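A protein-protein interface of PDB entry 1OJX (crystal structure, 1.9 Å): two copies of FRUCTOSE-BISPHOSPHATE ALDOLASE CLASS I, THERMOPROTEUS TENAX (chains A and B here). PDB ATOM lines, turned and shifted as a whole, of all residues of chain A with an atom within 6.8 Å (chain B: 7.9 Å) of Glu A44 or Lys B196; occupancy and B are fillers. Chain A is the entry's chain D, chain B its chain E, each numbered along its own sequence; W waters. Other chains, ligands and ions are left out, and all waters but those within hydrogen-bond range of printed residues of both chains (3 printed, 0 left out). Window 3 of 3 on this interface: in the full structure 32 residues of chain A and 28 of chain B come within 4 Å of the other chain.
The side-chain carboxylate (OE2) of Glu A44 lies within salt-bridge range of the side-chain amino group (NZ) of Lys B196 (3.6 Å). NZ of Lys A67 lies within salt-bridge range of OD1 of Asp B174 (3.1 Å). The backbone carbonyl oxygen of Ala B173 lies within hydrogen-bond range of the side-chain amino group of Lys A67. OH of Tyr A68 is in hydrogen-bond range of N of Lys B196, at 2.9 Å.
OD1 of Asn B3 sits at hydrogen-bond distance from N of Thr B5 (3.2 Å). The side-chain hydroxyl (OG1) of Thr B5 sits at hydrogen-bond distance from the backbone carbonyl oxygen (O) of Asp B174, at 2.8 Å. The side-chain carboxylate of Asp A42 lies within hydrogen-bond range of the backbone NH of Glu A44 (3.1 Å).
Thr B5 touches Lys A67 (OG1 to CE, 3.9 Å). Lys B196 touches Lys A67. Tyr A68 touches Gly B195 (OH to CA, 3.4 Å).
Glu A44 touches just one residue of chain B: Lys B196. Of the printed residues of chain B, Lys A67 touches Thr B5 (3.9 Å), Ala B173 (3.0 Å), Asp B174 (3.1 Å) and Lys B196 (3.4 Å). Printed residues of chain B within 4 Å of Tyr A68: Gly B195 and Lys B196. Glu B6 touches none of the printed residues of chain A. Printed residues of chain A within 4 Å of Gly B195: Tyr A68 (3.4 Å). Lys B196 touches just these residues of chain A: Glu A44 (3.6 Å), Lys A67 (3.4 Å) and Tyr A68 (2.9 Å). Val B199 touches none of the printed residues of chain A. The nearest printed residue of chain B that does not touch Glu A44 is Gly B195 (8.4 Å). The nearest printed residue of chain A that does not touch Gly B195 is Ala A41 (6.1 Å).
Hydrophobic or aromatic side chains of chain A within 4 Å of the printed part of chain B: Tyr A68. Of the 18 printed residues of chain B, 5 touch a printed residue of chain A. Printed residues of chain B that touch a printed residue of chain A: Thr B5, Ala B173, Asp B174, Gly B195 and Lys B196. Among the printed residues, 7 pairs touch across the chains. Among the printed residues, Asp or Glu carboxylates within 4 Å of a Lys or Arg side-chain nitrogen of the other chain: Glu A44 with Lys B196 (3.6 Å) and Lys A67 with Asp B174 (3.1 Å).
No position is printed for both chains.
Water W2 lies within hydrogen-bond range of O of Leu B169 (2.7 Å), O of Ala B173 (2.8 Å) and NZ of Lys A67 (2.9 Å). Water W1 lies within hydrogen-bond range of the side-chain carboxylate (OD1) of Asp A39 (2.9 Å) and the side-chain amino group (NZ) of Lys B192 (3.2 Å). Water W3 bridges O of Ala A41 (2.9 Å) and O of Lys B192 (2.9 Å).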
ATOM      1  N   TYR A  23     -20.711   0.848 -21.992  1.00  0.00           N
ATOM      2  CA  TYR A  23     -19.931   1.444 -23.081  1.00  0.00           C
ATOM      3  C   TYR A  23     -18.746   0.572 -23.483  1.00  0.00           C
ATOM      4  O   TYR A  23     -17.663   1.083 -23.747  1.00  0.00           O
ATOM      5  CB  TYR A  23     -19.444   2.830 -22.651  1.00  0.00           C
ATOM      6  CG  TYR A  23     -18.915   3.700 -23.771  1.00  0.00           C
ATOM      7  CD1 TYR A  23     -19.709   4.025 -24.861  1.00  0.00           C
ATOM      8  CD2 TYR A  23     -17.636   4.234 -23.716  1.00  0.00           C
ATOM      9  CE1 TYR A  23     -19.235   4.856 -25.895  1.00  0.00           C
ATOM     10  CE2 TYR A  23     -17.153   5.078 -24.746  1.00  0.00           C
ATOM     11  CZ  TYR A  23     -17.960   5.376 -25.828  1.00  0.00           C
ATOM     12  OH  TYR A  23     -17.502   6.207 -26.850  1.00  0.00           O
ATOM     13  N   ASP A  39     -21.285  12.232 -31.265  1.00  0.00           N
ATOM     14  CA  ASP A  39     -20.649  12.497 -29.966  1.00  0.00           C
ATOM     15  C   ASP A  39     -20.471  11.232 -29.110  1.00  0.00           C
ATOM     16  O   ASP A  39     -19.625  11.209 -28.211  1.00  0.00           O
ATOM     17  CB  ASP A  39     -21.446  13.521 -29.147  1.00  0.00           C
ATOM     18  CG  ASP A  39     -21.455  14.914 -29.770  1.00  0.00           C
ATOM     19  OD1 ASP A  39     -20.452  15.319 -30.402  1.00  0.00           O
ATOM     20  OD2 ASP A  39     -22.434  15.677 -29.667  1.00  0.00           O
ATOM     21  N   ALA A  41     -19.079   8.571 -29.801  1.00  0.00           N
ATOM     22  CA  ALA A  41     -17.721   8.048 -29.963  1.00  0.00           C
ATOM     23  C   ALA A  41     -16.721   8.605 -28.936  1.00  0.00           C
ATOM     24  O   ALA A  41     -15.611   8.102 -28.825  1.00  0.00           O
ATOM     25  CB  ALA A  41     -17.206   8.343 -31.395  1.00  0.00           C
ATOM     26  N   ASP A  42     -17.127   9.641 -28.207  1.00  0.00           N
ATOM     27  CA  ASP A  42     -16.291  10.363 -27.248  1.00  0.00           C
ATOM     28  C   ASP A  42     -16.621   9.906 -25.817  1.00  0.00           C
ATOM     29  O   ASP A  42     -17.696  10.202 -25.300  1.00  0.00           O
ATOM     30  CB  ASP A  42     -16.573  11.862 -27.414  1.00  0.00           C
ATOM     31  CG  ASP A  42     -15.668  12.754 -26.587  1.00  0.00           C
ATOM     32  OD1 ASP A  42     -14.824  12.269 -25.793  1.00  0.00           O
ATOM     33  OD2 ASP A  42     -15.763  13.997 -26.690  1.00  0.00           O
ATOM     34  N   PRO A  43     -15.714   9.180 -25.169  1.00  0.00           N
ATOM     35  CA  PRO A  43     -15.971   8.730 -23.796  1.00  0.00           C
ATOM     36  C   PRO A  43     -16.231   9.880 -22.810  1.00  0.00           C
ATOM     37  O   PRO A  43     -16.914   9.646 -21.815  1.00  0.00           O
ATOM     38  CB  PRO A  43     -14.693   7.984 -23.426  1.00  0.00           C
ATOM     39  CG  PRO A  43     -14.074   7.578 -24.748  1.00  0.00           C
ATOM     40  CD  PRO A  43     -14.413   8.705 -25.673  1.00  0.00           C
ATOM     41  N   GLU A  44     -15.691  11.072 -23.063  1.00  0.00           N
ATOM     42  CA  GLU A  44     -15.985  12.244 -22.224  1.00  0.00           C
ATOM     43  C   GLU A  44     -17.468  12.589 -22.296  1.00  0.00           C
ATOM     44  O   GLU A  44     -18.089  12.921 -21.290  1.00  0.00           O
ATOM     45  CB  GLU A  44     -15.185  13.475 -22.669  1.00  0.00           C
ATOM     46  CG  GLU A  44     -13.674  13.302 -22.667  1.00  0.00           C
ATOM     47  CD  GLU A  44     -12.916  14.620 -22.777  1.00  0.00           C
ATOM     48  OE1 GLU A  44     -13.532  15.706 -22.662  1.00  0.00           O
ATOM     49  OE2 GLU A  44     -11.681  14.556 -22.970  1.00  0.00           O
ATOM     50  N   TYR A  45     -18.015  12.590 -23.508  1.00  0.00           N
ATOM     51  CA  TYR A  45     -19.461  12.776 -23.693  1.00  0.00           C
ATOM     52  C   TYR A  45     -20.278  11.717 -22.928  1.00  0.00           C
ATOM     53  O   TYR A  45     -21.313  12.044 -22.353  1.00  0.00           O
ATOM     54  CB  TYR A  45     -19.811  12.811 -25.187  1.00  0.00           C
ATOM     55  CG  TYR A  45     -21.293  12.684 -25.518  1.00  0.00           C
ATOM     56  CD1 TYR A  45     -22.122  13.801 -25.542  1.00  0.00           C
ATOM     57  CD2 TYR A  45     -21.851  11.445 -25.824  1.00  0.00           C
ATOM     58  CE1 TYR A  45     -23.471  13.688 -25.866  1.00  0.00           C
ATOM     59  CE2 TYR A  45     -23.187  11.321 -26.135  1.00  0.00           C
ATOM     60  CZ  TYR A  45     -23.989  12.441 -26.154  1.00  0.00           C
ATOM     61  OH  TYR A  45     -25.302  12.313 -26.478  1.00  0.00           O
ATOM     62  N   ILE A  46     -19.804  10.464 -22.898  1.00  0.00           N
ATOM     63  CA  ILE A  46     -20.492   9.375 -22.169  1.00  0.00           C
ATOM     64  C   ILE A  46     -20.497   9.573 -20.637  1.00  0.00           C
ATOM     65  O   ILE A  46     -21.501   9.323 -19.980  1.00  0.00           O
ATOM     66  CB  ILE A  46     -19.867   7.995 -22.515  1.00  0.00           C
ATOM     67  CG1 ILE A  46     -19.997   7.668 -24.012  1.00  0.00           C
ATOM     68  CG2 ILE A  46     -20.489   6.880 -21.659  1.00  0.00           C
ATOM     69  CD1 ILE A  46     -21.414   7.547 -24.532  1.00  0.00           C
ATOM     70  N   LEU A  47     -19.382  10.023 -20.072  1.00  0.00           N
ATOM     71  CA  LEU A  47     -19.313  10.311 -18.638  1.00  0.00           C
ATOM     72  C   LEU A  47     -20.249  11.456 -18.236  1.00  0.00           C
ATOM     73  O   LEU A  47     -20.915  11.385 -17.196  1.00  0.00           O
ATOM     74  CB  LEU A  47     -17.870  10.618 -18.217  1.00  0.00           C
ATOM     75  CG  LEU A  47     -16.943   9.387 -18.123  1.00  0.00           C
ATOM     76  CD1 LEU A  47     -15.493   9.819 -18.076  1.00  0.00           C
ATOM     77  CD2 LEU A  47     -17.268   8.541 -16.899  1.00  0.00           C
ATOM     78  N   ARG A  48     -20.313  12.499 -19.060  1.00  0.00           N
ATOM     79  CA  ARG A  48     -21.239  13.622 -18.819  1.00  0.00           C
ATOM     80  C   ARG A  48     -22.698  13.185 -18.838  1.00  0.00           C
ATOM     81  O   ARG A  48     -23.498  13.635 -18.030  1.00  0.00           O
ATOM     82  CB  ARG A  48     -21.051  14.732 -19.854  1.00  0.00           C
ATOM     83  CG  ARG A  48     -19.829  15.610 -19.650  1.00  0.00           C
ATOM     84  CD  ARG A  48     -19.947  16.973 -20.365  1.00  0.00           C
ATOM     85  NE  ARG A  48     -19.793  16.807 -21.810  1.00  0.00           N
ATOM     86  CZ  ARG A  48     -18.629  16.691 -22.444  1.00  0.00           C
ATOM     87  NH1 ARG A  48     -17.476  16.741 -21.774  1.00  0.00           N
ATOM     88  NH2 ARG A  48     -18.616  16.524 -23.766  1.00  0.00           N
ATOM     89  N   LEU A  49     -23.034  12.313 -19.773  1.00  0.00           N
ATOM     90  CA  LEU A  49     -24.393  11.796 -19.919  1.00  0.00           C
ATOM     91  C   LEU A  49     -24.817  10.997 -18.679  1.00  0.00           C
ATOM     92  O   LEU A  49     -25.935  11.152 -18.183  1.00  0.00           O
ATOM     93  CB  LEU A  49     -24.455  10.924 -21.165  1.00  0.00           C
ATOM     94  CG  LEU A  49     -25.725  10.491 -21.847  1.00  0.00           C
ATOM     95  CD1 LEU A  49     -26.608  11.675 -22.178  1.00  0.00           C
ATOM     96  CD2 LEU A  49     -25.339   9.723 -23.128  1.00  0.00           C
ATOM     97  N   PHE A  60     -16.615   0.436 -18.707  1.00  0.00           N
ATOM     98  CA  PHE A  60     -15.535   0.696 -19.683  1.00  0.00           C
ATOM     99  C   PHE A  60     -14.571  -0.485 -19.739  1.00  0.00           C
ATOM    100  O   PHE A  60     -14.297  -1.097 -18.715  1.00  0.00           O
ATOM    101  CB  PHE A  60     -14.630   1.857 -19.234  1.00  0.00           C
ATOM    102  CG  PHE A  60     -15.219   3.253 -19.350  1.00  0.00           C
ATOM    103  CD1 PHE A  60     -16.373   3.523 -20.064  1.00  0.00           C
ATOM    104  CD2 PHE A  60     -14.564   4.309 -18.716  1.00  0.00           C
ATOM    105  CE1 PHE A  60     -16.855   4.813 -20.147  1.00  0.00           C
ATOM    106  CE2 PHE A  60     -15.039   5.596 -18.797  1.00  0.00           C
ATOM    107  CZ  PHE A  60     -16.194   5.853 -19.515  1.00  0.00           C
ATOM    108  N   LYS A  67      -7.412   6.182 -20.337  1.00  0.00           N
ATOM    109  CA  LYS A  67      -7.355   7.482 -21.056  1.00  0.00           C
ATOM    110  C   LYS A  67      -8.403   8.519 -20.631  1.00  0.00           C
ATOM    111  O   LYS A  67      -8.196   9.750 -20.817  1.00  0.00           O
ATOM    112  CB  LYS A  67      -7.491   7.287 -22.569  1.00  0.00           C
ATOM    113  CG  LYS A  67      -6.168   7.206 -23.328  1.00  0.00           C
ATOM    114  CD  LYS A  67      -5.441   5.979 -22.968  1.00  0.00           C
ATOM    115  CE  LYS A  67      -4.101   5.848 -23.692  1.00  0.00           C
ATOM    116  NZ  LYS A  67      -3.614   4.469 -23.510  1.00  0.00           N
ATOM    117  N   TYR A  68      -9.532   8.052 -20.110  1.00  0.00           N
ATOM    118  CA  TYR A  68     -10.681   8.920 -19.930  1.00  0.00           C
ATOM    119  C   TYR A  68     -11.332   8.952 -18.551  1.00  0.00           C
ATOM    120  O   TYR A  68     -11.979   9.946 -18.236  1.00  0.00           O
ATOM    121  CB  TYR A  68     -11.768   8.621 -20.968  1.00  0.00           C
ATOM    122  CG  TYR A  68     -11.367   8.965 -22.385  1.00  0.00           C
ATOM    123  CD1 TYR A  68     -11.562  10.259 -22.907  1.00  0.00           C
ATOM    124  CD2 TYR A  68     -10.792   8.008 -23.204  1.00  0.00           C
ATOM    125  CE1 TYR A  68     -11.186  10.564 -24.222  1.00  0.00           C
ATOM    126  CE2 TYR A  68     -10.421   8.300 -24.504  1.00  0.00           C
ATOM    127  CZ  TYR A  68     -10.621   9.563 -25.012  1.00  0.00           C
ATOM    128  OH  TYR A  68     -10.226   9.806 -26.308  1.00  0.00           O
ATOM    129  N   ASN B   3       1.749   9.592 -18.171  1.00  0.00           N
ATOM    130  CA  ASN B   3       0.984   9.520 -19.443  1.00  0.00           C
ATOM    131  C   ASN B   3       1.898   9.057 -20.588  1.00  0.00           C
ATOM    132  O   ASN B   3       2.728   9.826 -21.080  1.00  0.00           O
ATOM    133  CB  ASN B   3       0.398  10.897 -19.744  1.00  0.00           C
ATOM    134  CG  ASN B   3      -0.561  10.866 -20.907  1.00  0.00           C
ATOM    135  OD1 ASN B   3      -0.280  10.237 -21.919  1.00  0.00           O
ATOM    136  ND2 ASN B   3      -1.708  11.519 -20.757  1.00  0.00           N
ATOM    137  N   THR B   5       1.236   8.160 -23.748  1.00  0.00           N
ATOM    138  CA  THR B   5       0.994   8.790 -25.047  1.00  0.00           C
ATOM    139  C   THR B   5       1.820  10.088 -25.131  1.00  0.00           C
ATOM    140  O   THR B   5       2.476  10.358 -26.143  1.00  0.00           O
ATOM    141  CB  THR B   5      -0.504   9.069 -25.240  1.00  0.00           C
ATOM    142  OG1 THR B   5      -1.205   7.832 -25.456  1.00  0.00           O
ATOM    143  CG2 THR B   5      -0.762   9.881 -26.503  1.00  0.00           C
ATOM    144  N   GLU B   6       1.818  10.864 -24.046  1.00  0.00           N
ATOM    145  CA  GLU B   6       2.601  12.094 -23.994  1.00  0.00           C
ATOM    146  C   GLU B   6       4.096  11.803 -24.157  1.00  0.00           C
ATOM    147  O   GLU B   6       4.780  12.522 -24.900  1.00  0.00           O
ATOM    148  CB  GLU B   6       2.303  12.883 -22.712  1.00  0.00           C
ATOM    149  CG  GLU B   6       0.887  13.447 -22.715  1.00  0.00           C
ATOM    150  CD  GLU B   6       0.545  14.291 -21.492  1.00  0.00           C
ATOM    151  OE1 GLU B   6       1.073  14.033 -20.388  1.00  0.00           O
ATOM    152  OE2 GLU B   6      -0.281  15.219 -21.647  1.00  0.00           O
ATOM    153  N   LEU B   9       4.788  11.038 -27.852  1.00  0.00           N
ATOM    154  CA  LEU B   9       4.769  12.221 -28.721  1.00  0.00           C
ATOM    155  C   LEU B   9       6.054  13.060 -28.576  1.00  0.00           C
ATOM    156  O   LEU B   9       6.514  13.662 -29.540  1.00  0.00           O
ATOM    157  CB  LEU B   9       3.523  13.064 -28.437  1.00  0.00           C
ATOM    158  CG  LEU B   9       2.180  12.438 -28.838  1.00  0.00           C
ATOM    159  CD1 LEU B   9       1.016  13.243 -28.251  1.00  0.00           C
ATOM    160  CD2 LEU B   9       2.065  12.349 -30.353  1.00  0.00           C
ATOM    161  N   LEU B 169      -7.500   1.445 -29.221  1.00  0.00           N
ATOM    162  CA  LEU B 169      -7.808   2.330 -28.080  1.00  0.00           C
ATOM    163  C   LEU B 169      -8.349   1.555 -26.872  1.00  0.00           C
ATOM    164  O   LEU B 169      -7.864   1.735 -25.745  1.00  0.00           O
ATOM    165  CB  LEU B 169      -8.823   3.418 -28.480  1.00  0.00           C
ATOM    166  CG  LEU B 169      -9.493   4.273 -27.378  1.00  0.00           C
ATOM    167  CD1 LEU B 169      -8.499   5.160 -26.597  1.00  0.00           C
ATOM    168  CD2 LEU B 169     -10.557   5.124 -27.987  1.00  0.00           C
ATOM    169  N   ALA B 173      -3.608   0.709 -26.233  1.00  0.00           N
ATOM    170  CA  ALA B 173      -2.522   1.312 -27.018  1.00  0.00           C
ATOM    171  C   ALA B 173      -2.271   2.762 -26.617  1.00  0.00           C
ATOM    172  O   ALA B 173      -3.215   3.513 -26.329  1.00  0.00           O
ATOM    173  CB  ALA B 173      -2.829   1.265 -28.469  1.00  0.00           C
ATOM    174  N   ASP B 174      -1.001   3.144 -26.599  1.00  0.00           N
ATOM    175  CA  ASP B 174      -0.610   4.554 -26.413  1.00  0.00           C
ATOM    176  C   ASP B 174      -0.426   5.297 -27.756  1.00  0.00           C
ATOM    177  O   ASP B 174      -0.441   6.537 -27.819  1.00  0.00           O
ATOM    178  CB  ASP B 174       0.654   4.589 -25.576  1.00  0.00           C
ATOM    179  CG  ASP B 174       0.470   3.866 -24.246  1.00  0.00           C
ATOM    180  OD1 ASP B 174      -0.569   4.135 -23.581  1.00  0.00           O
ATOM    181  OD2 ASP B 174       1.267   2.995 -23.818  1.00  0.00           O
ATOM    182  N   ALA B 175      -0.178   4.517 -28.798  1.00  0.00           N
ATOM    183  CA  ALA B 175      -0.269   4.942 -30.202  1.00  0.00           C
ATOM    184  C   ALA B 175      -0.587   3.712 -31.041  1.00  0.00           C
ATOM    185  O   ALA B 175      -0.436   2.570 -30.580  1.00  0.00           O
ATOM    186  CB  ALA B 175       1.016   5.556 -30.677  1.00  0.00           C
ATOM    187  N   MET B 176      -1.005   3.938 -32.277  1.00  0.00           N
ATOM    188  CA  MET B 176      -1.392   2.832 -33.156  1.00  0.00           C
ATOM    189  C   MET B 176      -0.990   3.053 -34.612  1.00  0.00           C
ATOM    190  O   MET B 176      -0.768   4.180 -35.050  1.00  0.00           O
ATOM    191  CB  MET B 176      -2.903   2.579 -33.073  1.00  0.00           C
ATOM    192  CG  MET B 176      -3.759   3.639 -33.757  1.00  0.00           C
ATOM    193  SD  MET B 176      -5.552   3.435 -33.542  1.00  0.00           S
ATOM    194  CE  MET B 176      -5.838   3.902 -31.857  1.00  0.00           C
ATOM    195  N   VAL B 191      -9.602   8.169 -37.405  1.00  0.00           N
ATOM    196  CA  VAL B 191      -8.836   9.041 -36.533  1.00  0.00           C
ATOM    197  C   VAL B 191      -9.698   9.539 -35.369  1.00  0.00           C
ATOM    198  O   VAL B 191      -9.223   9.591 -34.227  1.00  0.00           O
ATOM    199  CB  VAL B 191      -8.237  10.230 -37.320  1.00  0.00           C
ATOM    200  CG1 VAL B 191      -7.692  11.301 -36.371  1.00  0.00           C
ATOM    201  CG2 VAL B 191      -7.145   9.752 -38.263  1.00  0.00           C
ATOM    202  N   LYS B 192     -10.956   9.892 -35.653  1.00  0.00           N
ATOM    203  CA  LYS B 192     -11.870  10.401 -34.625  1.00  0.00           C
ATOM    204  C   LYS B 192     -12.168   9.355 -33.554  1.00  0.00           C
ATOM    205  O   LYS B 192     -12.115   9.663 -32.375  1.00  0.00           O
ATOM    206  CB  LYS B 192     -13.184  10.911 -35.235  1.00  0.00           C
ATOM    207  CG  LYS B 192     -14.221  11.361 -34.188  1.00  0.00           C
ATOM    208  CD  LYS B 192     -15.028  12.571 -34.637  1.00  0.00           C
ATOM    209  CE  LYS B 192     -16.365  12.711 -33.880  1.00  0.00           C
ATOM    210  NZ  LYS B 192     -16.196  13.122 -32.438  1.00  0.00           N
ATOM    211  N   VAL B 193     -12.446   8.110 -33.948  1.00  0.00           N
ATOM    212  CA  VAL B 193     -12.842   7.095 -32.972  1.00  0.00           C
ATOM    213  C   VAL B 193     -11.670   6.592 -32.141  1.00  0.00           C
ATOM    214  O   VAL B 193     -11.884   5.979 -31.090  1.00  0.00           O
ATOM    215  CB  VAL B 193     -13.607   5.892 -33.604  1.00  0.00           C
ATOM    216  CG1 VAL B 193     -14.852   6.385 -34.329  1.00  0.00           C
ATOM    217  CG2 VAL B 193     -12.715   5.070 -34.525  1.00  0.00           C
ATOM    218  N   ALA B 194     -10.447   6.866 -32.608  1.00  0.00           N
ATOM    219  CA  ALA B 194      -9.232   6.595 -31.848  1.00  0.00           C
ATOM    220  C   ALA B 194      -9.070   7.582 -30.701  1.00  0.00           C
ATOM    221  O   ALA B 194      -8.232   7.381 -29.826  1.00  0.00           O
ATOM    222  CB  ALA B 194      -8.003   6.676 -32.755  1.00  0.00           C
ATOM    223  N   GLY B 195      -9.824   8.677 -30.733  1.00  0.00           N
ATOM    224  CA  GLY B 195      -9.778   9.653 -29.658  1.00  0.00           C
ATOM    225  C   GLY B 195      -8.391  10.215 -29.358  1.00  0.00           C
ATOM    226  O   GLY B 195      -7.709  10.695 -30.261  1.00  0.00           O
ATOM    227  N   LYS B 196      -7.978  10.125 -28.088  1.00  0.00           N
ATOM    228  CA  LYS B 196      -6.710  10.674 -27.585  1.00  0.00           C
ATOM    229  C   LYS B 196      -5.460   9.933 -28.074  1.00  0.00           C
ATOM    230  O   LYS B 196      -4.337  10.397 -27.844  1.00  0.00           O
ATOM    231  CB  LYS B 196      -6.674  10.628 -26.026  1.00  0.00           C
ATOM    232  CG  LYS B 196      -7.537  11.631 -25.290  1.00  0.00           C
ATOM    233  CD  LYS B 196      -7.313  11.485 -23.771  1.00  0.00           C
ATOM    234  CE  LYS B 196      -8.208  12.395 -22.932  1.00  0.00           C
ATOM    235  NZ  LYS B 196      -8.228  13.814 -23.405  1.00  0.00           N
ATOM    236  N   VAL B 197      -5.629   8.768 -28.689  1.00  0.00           N
ATOM    237  CA  VAL B 197      -4.492   7.951 -29.121  1.00  0.00           C
ATOM    238  C   VAL B 197      -4.112   8.303 -30.573  1.00  0.00           C
ATOM    239  O   VAL B 197      -4.960   8.215 -31.483  1.00  0.00           O
ATOM    240  CB  VAL B 197      -4.807   6.442 -29.018  1.00  0.00           C
ATOM    241  CG1 VAL B 197      -3.633   5.608 -29.518  1.00  0.00           C
ATOM    242  CG2 VAL B 197      -5.145   6.054 -27.566  1.00  0.00           C
ATOM    243  N   PRO B 198      -2.869   8.727 -30.815  1.00  0.00           N
ATOM    244  CA  PRO B 198      -2.490   9.148 -32.174  1.00  0.00           C
ATOM    245  C   PRO B 198      -2.406   7.977 -33.148  1.00  0.00           C
ATOM    246  O   PRO B 198      -2.116   6.850 -32.750  1.00  0.00           O
ATOM    247  CB  PRO B 198      -1.122   9.805 -31.976  1.00  0.00           C
ATOM    248  CG  PRO B 198      -0.576   9.149 -30.757  1.00  0.00           C
ATOM    249  CD  PRO B 198      -1.766   8.921 -29.857  1.00  0.00           C
ATOM    250  N   VAL B 199      -2.653   8.282 -34.421  1.00  0.00           N
ATOM    251  CA  VAL B 199      -2.715   7.306 -35.493  1.00  0.00           C
ATOM    252  C   VAL B 199      -1.613   7.547 -36.524  1.00  0.00           C
ATOM    253  O   VAL B 199      -1.423   8.673 -37.019  1.00  0.00           O
ATOM    254  CB  VAL B 199      -4.074   7.389 -36.206  1.00  0.00           C
ATOM    255  CG1 VAL B 199      -4.077   6.566 -37.507  1.00  0.00           C
ATOM    256  CG2 VAL B 199      -5.166   6.918 -35.273  1.00  0.00           C
HETATM  257  O   HOH W   1     -19.027  14.558 -32.787  1.00  0.00           O
HETATM  258  O   HOH W   2      -5.642   3.105 -24.994  1.00  0.00           O
HETATM  259  O   HOH W   3     -13.709   9.960 -29.974  1.00  0.00           O
